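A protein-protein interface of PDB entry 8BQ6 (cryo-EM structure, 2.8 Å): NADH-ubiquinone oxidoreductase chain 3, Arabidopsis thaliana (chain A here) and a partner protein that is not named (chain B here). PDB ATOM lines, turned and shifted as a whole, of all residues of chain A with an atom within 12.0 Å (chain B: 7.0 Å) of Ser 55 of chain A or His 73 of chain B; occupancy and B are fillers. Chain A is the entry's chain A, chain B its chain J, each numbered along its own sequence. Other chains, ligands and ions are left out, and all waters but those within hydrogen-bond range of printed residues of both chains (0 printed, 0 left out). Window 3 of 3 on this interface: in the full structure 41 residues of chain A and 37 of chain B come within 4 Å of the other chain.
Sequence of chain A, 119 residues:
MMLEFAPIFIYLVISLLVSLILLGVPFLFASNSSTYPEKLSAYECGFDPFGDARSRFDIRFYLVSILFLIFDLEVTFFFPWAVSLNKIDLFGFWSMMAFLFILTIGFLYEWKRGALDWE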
ATOM      1  N   SER A  55       2.689 -22.121 -19.244  1.00  0.00           N
ATOM      2  CA  SER A  55       3.430 -23.371 -19.187  1.00  0.00           C
ATOM      3  C   SER A  55       4.138 -23.592 -17.848  1.00  0.00           C
ATOM      4  O   SER A  55       5.247 -24.123 -17.818  1.00  0.00           O
ATOM      5  CB  SER A  55       4.460 -23.414 -20.317  1.00  0.00           C
ATOM      6  OG  SER A  55       5.489 -22.464 -20.092  1.00  0.00           O
ATOM      7  N   ARG A  56       3.515 -23.196 -16.738  1.00  0.00           N
ATOM      8  CA  ARG A  56       4.139 -23.330 -15.419  1.00  0.00           C
ATOM      9  C   ARG A  56       3.074 -23.636 -14.372  1.00  0.00           C
ATOM     10  O   ARG A  56       2.397 -22.736 -13.870  1.00  0.00           O
ATOM     11  CB  ARG A  56       4.920 -22.087 -15.058  1.00  0.00           C
ATOM     12  CG  ARG A  56       6.072 -21.792 -16.006  1.00  0.00           C
ATOM     13  CD  ARG A  56       7.150 -22.878 -15.980  1.00  0.00           C
ATOM     14  NE  ARG A  56       7.775 -23.045 -14.670  1.00  0.00           N
ATOM     15  CZ  ARG A  56       8.756 -22.288 -14.195  1.00  0.00           C
ATOM     16  NH1 ARG A  56       9.315 -21.336 -14.926  1.00  0.00           N
ATOM     17  NH2 ARG A  56       9.182 -22.486 -12.950  1.00  0.00           N
ATOM     18  N   PHE A  57       2.956 -24.908 -14.019  1.00  0.00           N
ATOM     19  CA  PHE A  57       1.870 -25.350 -13.161  1.00  0.00           C
ATOM     20  C   PHE A  57       2.215 -25.113 -11.697  1.00  0.00           C
ATOM     21  O   PHE A  57       3.209 -25.645 -11.195  1.00  0.00           O
ATOM     22  CB  PHE A  57       1.577 -26.823 -13.403  1.00  0.00           C
ATOM     23  CG  PHE A  57       0.259 -27.241 -12.877  1.00  0.00           C
ATOM     24  CD1 PHE A  57       0.105 -27.573 -11.547  1.00  0.00           C
ATOM     25  CD2 PHE A  57      -0.846 -27.240 -13.696  1.00  0.00           C
ATOM     26  CE1 PHE A  57      -1.118 -27.930 -11.055  1.00  0.00           C
ATOM     27  CE2 PHE A  57      -2.071 -27.593 -13.208  1.00  0.00           C
ATOM     28  CZ  PHE A  57      -2.209 -27.939 -11.887  1.00  0.00           C
ATOM     29  N   ASP A  58       1.379 -24.351 -11.000  1.00  0.00           N
ATOM     30  CA  ASP A  58       1.562 -24.102  -9.575  1.00  0.00           C
ATOM     31  C   ASP A  58       0.524 -24.890  -8.785  1.00  0.00           C
ATOM     32  O   ASP A  58      -0.659 -24.534  -8.777  1.00  0.00           O
ATOM     33  CB  ASP A  58       1.473 -22.614  -9.257  1.00  0.00           C
ATOM     34  CG  ASP A  58       1.945 -22.303  -7.856  1.00  0.00           C
ATOM     35  OD1 ASP A  58       2.153 -23.251  -7.075  1.00  0.00           O
ATOM     36  OD2 ASP A  58       2.127 -21.116  -7.532  1.00  0.00           O
ATOM     37  N   ILE A  59       0.980 -25.928  -8.079  1.00  0.00           N
ATOM     38  CA  ILE A  59       0.071 -26.789  -7.331  1.00  0.00           C
ATOM     39  C   ILE A  59      -0.643 -26.055  -6.209  1.00  0.00           C
ATOM     40  O   ILE A  59      -1.668 -26.537  -5.721  1.00  0.00           O
ATOM     41  CB  ILE A  59       0.803 -28.015  -6.742  1.00  0.00           C
ATOM     42  CG1 ILE A  59       1.818 -27.562  -5.688  1.00  0.00           C
ATOM     43  CG2 ILE A  59       1.417 -28.876  -7.842  1.00  0.00           C
ATOM     44  CD1 ILE A  59       2.358 -28.664  -4.832  1.00  0.00           C
ATOM     45  N   PHE A  61      -2.390 -23.471  -6.292  1.00  0.00           N
ATOM     46  CA  PHE A  61      -3.724 -23.055  -6.705  1.00  0.00           C
ATOM     47  C   PHE A  61      -4.699 -24.226  -6.691  1.00  0.00           C
ATOM     48  O   PHE A  61      -5.869 -24.065  -6.320  1.00  0.00           O
ATOM     49  CB  PHE A  61      -3.656 -22.391  -8.076  1.00  0.00           C
ATOM     50  CG  PHE A  61      -2.943 -21.079  -8.056  1.00  0.00           C
ATOM     51  CD1 PHE A  61      -3.518 -19.983  -7.446  1.00  0.00           C
ATOM     52  CD2 PHE A  61      -1.692 -20.941  -8.619  1.00  0.00           C
ATOM     53  CE1 PHE A  61      -2.869 -18.777  -7.408  1.00  0.00           C
ATOM     54  CE2 PHE A  61      -1.041 -19.731  -8.582  1.00  0.00           C
ATOM     55  CZ  PHE A  61      -1.631 -18.649  -7.975  1.00  0.00           C
ATOM     56  N   VAL B  68      -7.216 -25.863 -12.877  1.00  0.00           N
ATOM     57  CA  VAL B  68      -6.357 -26.939 -13.351  1.00  0.00           C
ATOM     58  C   VAL B  68      -6.194 -26.866 -14.864  1.00  0.00           C
ATOM     59  O   VAL B  68      -5.075 -26.930 -15.383  1.00  0.00           O
ATOM     60  CB  VAL B  68      -6.900 -28.310 -12.918  1.00  0.00           C
ATOM     61  CG1 VAL B  68      -6.153 -29.397 -13.656  1.00  0.00           C
ATOM     62  CG2 VAL B  68      -6.761 -28.487 -11.424  1.00  0.00           C
ATOM     63  N   VAL B  69      -7.301 -26.730 -15.597  1.00  0.00           N
ATOM     64  CA  VAL B  69      -7.217 -26.762 -17.053  1.00  0.00           C
ATOM     65  C   VAL B  69      -6.403 -25.591 -17.578  1.00  0.00           C
ATOM     66  O   VAL B  69      -5.569 -25.759 -18.474  1.00  0.00           O
ATOM     67  CB  VAL B  69      -8.626 -26.810 -17.666  1.00  0.00           C
ATOM     68  CG1 VAL B  69      -8.579 -26.438 -19.120  1.00  0.00           C
ATOM     69  CG2 VAL B  69      -9.178 -28.210 -17.540  1.00  0.00           C
ATOM     70  N   MET B  70      -6.609 -24.401 -17.021  1.00  0.00           N
ATOM     71  CA  MET B  70      -5.898 -23.214 -17.479  1.00  0.00           C
ATOM     72  C   MET B  70      -4.394 -23.346 -17.272  1.00  0.00           C
ATOM     73  O   MET B  70      -3.608 -23.015 -18.166  1.00  0.00           O
ATOM     74  CB  MET B  70      -6.432 -21.999 -16.737  1.00  0.00           C
ATOM     75  CG  MET B  70      -7.475 -21.248 -17.490  1.00  0.00           C
ATOM     76  SD  MET B  70      -8.268 -20.005 -16.477  1.00  0.00           S
ATOM     77  CE  MET B  70      -9.633 -19.583 -17.545  1.00  0.00           C
ATOM     78  N   MET B  71      -3.972 -23.827 -16.102  1.00  0.00           N
ATOM     79  CA  MET B  71      -2.546 -23.957 -15.841  1.00  0.00           C
ATOM     80  C   MET B  71      -1.901 -25.092 -16.624  1.00  0.00           C
ATOM     81  O   MET B  71      -0.672 -25.115 -16.746  1.00  0.00           O
ATOM     82  CB  MET B  71      -2.283 -24.161 -14.347  1.00  0.00           C
ATOM     83  CG  MET B  71      -2.684 -23.003 -13.462  1.00  0.00           C
ATOM     84  SD  MET B  71      -2.247 -23.287 -11.735  1.00  0.00           S
ATOM     85  CE  MET B  71      -3.498 -24.464 -11.234  1.00  0.00           C
ATOM     86  N   PHE B  72      -2.690 -26.022 -17.161  1.00  0.00           N
ATOM     87  CA  PHE B  72      -2.146 -27.168 -17.929  1.00  0.00           C
ATOM     88  C   PHE B  72      -1.708 -26.726 -19.326  1.00  0.00           C
ATOM     89  O   PHE B  72      -0.870 -27.440 -19.888  1.00  0.00           O
ATOM     90  CB  PHE B  72      -3.195 -28.274 -18.084  1.00  0.00           C
ATOM     91  CG  PHE B  72      -3.171 -29.392 -17.074  1.00  0.00           C
ATOM     92  CD1 PHE B  72      -4.204 -30.314 -17.029  1.00  0.00           C
ATOM     93  CD2 PHE B  72      -2.126 -29.534 -16.179  1.00  0.00           C
ATOM     94  CE1 PHE B  72      -4.196 -31.349 -16.108  1.00  0.00           C
ATOM     95  CE2 PHE B  72      -2.123 -30.563 -15.250  1.00  0.00           C
ATOM     96  CZ  PHE B  72      -3.156 -31.468 -15.216  1.00  0.00           C
ATOM     97  N   HIS B  73      -2.254 -25.624 -19.863  1.00  0.00           N
ATOM     98  CA  HIS B  73      -1.943 -25.144 -21.213  1.00  0.00           C
ATOM     99  C   HIS B  73      -1.928 -26.293 -22.220  1.00  0.00           C
ATOM    100  O   HIS B  73      -0.942 -26.520 -22.923  1.00  0.00           O
ATOM    101  CB  HIS B  73      -0.613 -24.384 -21.238  1.00  0.00           C
ATOM    102  CG  HIS B  73      -0.641 -23.085 -20.494  1.00  0.00           C
ATOM    103  ND1 HIS B  73      -0.149 -22.952 -19.214  1.00  0.00           N
ATOM    104  CD2 HIS B  73      -1.102 -21.862 -20.848  1.00  0.00           C
ATOM    105  CE1 HIS B  73      -0.309 -21.704 -18.810  1.00  0.00           C
ATOM    106  NE2 HIS B  73      -0.884 -21.022 -19.783  1.00  0.00           N
ATOM    107  N   ILE B  74      -3.030 -27.041 -22.269  1.00  0.00           N
ATOM    108  CA  ILE B  74      -3.113 -28.168 -23.191  1.00  0.00           C
ATOM    109  C   ILE B  74      -2.971 -27.656 -24.615  1.00  0.00           C
ATOM    110  O   ILE B  74      -3.535 -26.616 -24.980  1.00  0.00           O
ATOM    111  CB  ILE B  74      -4.426 -28.941 -23.000  1.00  0.00           C
ATOM    112  CG1 ILE B  74      -4.424 -29.668 -21.660  1.00  0.00           C
ATOM    113  CG2 ILE B  74      -4.630 -29.955 -24.110  1.00  0.00           C
ATOM    114  CD1 ILE B  74      -5.696 -29.506 -20.907  1.00  0.00           C
ATOM    115  N   GLN B  75      -2.180 -28.362 -25.413  1.00  0.00           N
ATOM    116  CA  GLN B  75      -2.034 -28.046 -26.824  1.00  0.00           C
ATOM    117  C   GLN B  75      -3.034 -28.851 -27.636  1.00  0.00           C
ATOM    118  O   GLN B  75      -3.276 -30.030 -27.358  1.00  0.00           O
ATOM    119  CB  GLN B  75      -0.607 -28.321 -27.298  1.00  0.00           C
ATOM    120  CG  GLN B  75       0.481 -27.741 -26.390  1.00  0.00           C
ATOM    121  CD  GLN B  75       0.459 -26.218 -26.309  1.00  0.00           C
ATOM    122  OE1 GLN B  75      -0.370 -25.554 -26.933  1.00  0.00           O
ATOM    123  NE2 GLN B  75       1.383 -25.658 -25.541  1.00  0.00           N
ATOM    124  N   ILE B  76      -3.613 -28.204 -28.649  1.00  0.00           N
ATOM    125  CA  ILE B  76      -4.755 -28.783 -29.347  1.00  0.00           C
ATOM    126  C   ILE B  76      -4.361 -30.063 -30.067  1.00  0.00           C
ATOM    127  O   ILE B  76      -5.217 -30.901 -30.368  1.00  0.00           O
ATOM    128  CB  ILE B  76      -5.371 -27.745 -30.308  1.00  0.00           C
ATOM    129  CG1 ILE B  76      -6.790 -28.151 -30.699  1.00  0.00           C
ATOM    130  CG2 ILE B  76      -4.526 -27.591 -31.556  1.00  0.00           C
ATOM    131  CD1 ILE B  76      -7.748 -28.178 -29.551  1.00  0.00           C
ATOM    132  N   GLU B  78      -2.371 -32.549 -28.902  1.00  0.00           N
ATOM    133  CA  GLU B  78      -2.360 -33.671 -27.973  1.00  0.00           C
ATOM    134  C   GLU B  78      -3.734 -34.281 -27.745  1.00  0.00           C
ATOM    135  O   GLU B  78      -3.819 -35.405 -27.242  1.00  0.00           O
ATOM    136  CB  GLU B  78      -1.800 -33.224 -26.625  1.00  0.00           C
ATOM    137  CG  GLU B  78      -0.466 -32.529 -26.716  1.00  0.00           C
ATOM    138  CD  GLU B  78       0.256 -32.513 -25.393  1.00  0.00           C
ATOM    139  OE1 GLU B  78      -0.402 -32.241 -24.372  1.00  0.00           O
ATOM    140  OE2 GLU B  78       1.476 -32.777 -25.372  1.00  0.00           O
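Ser 55 of chain A touches just one residue of chain B: His 73.
Printed residues of chain B within 4 Å of Phe 61 of chain A: Met 71 (3.8 Å).
Printed residues of chain A within 4 Å of Val 68 of chain B: Phe 57.
Of the printed residues of chain A, Met 71 of chain B touches Phe 57, Asp 58 and Phe 61.
Phe 72 of chain B touches just one residue of chain A: Phe 57.
His 73 of chain B touches just one residue of chain A: Ser 55.
No residue of chain A comes within 4 Å of Gln 75 of chain B.
Glu 78 of chain B touches none of the printed residues of chain A.
The nearest residue of chain A that does not touch His 73 of chain B is Arg 56 of chain A (4.4 Å).
The nearest printed residue of chain B that does not touch Phe 61 of chain A is Val 68 of chain B (6.7 Å).
Of the 6 printed residues of chain A, 4 touch a printed residue of chain B.
Hydrophobic or aromatic side chains of chain A within 4 Å of the printed part of chain B: Phe 57 and Phe 61.
Along chain A the printed residues that touch a printed residue of chain B span positions 55 to 61.
Hydrophobic or aromatic side chains of chain B that line the printed part of chain A: Met 71, Phe 72 and His 73.
Among the printed residues, no Asp or Glu carboxylate lies within 4 Å of a Lys or Arg side-chain nitrogen of the other chain.
Among the printed residues, merely in contact across the chains: Phe 57 of chain A with Met 71 of chain B, Phe 57 of chain A with Phe 72 of chain B, Phe 57 of chain A with Val 68 of chain B and Phe 61 of chain A with Met 71 of chain B.
The backbone carbonyl oxygen (O) of Met 71 of chain B is in hydrogen-bond range of a ring nitrogen (ND1) of His 73 of chain B (3.3 Å).
N of Ser 55 of chain A is in hydrogen-bond range of ND1 of His 73 of chain B (3.0 Å).
The backbone carbonyl oxygen (O) of Asp 58 of chain A lies close to the side-chain sulfur (SD) of Met 71 of chain B (3.6 Å).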
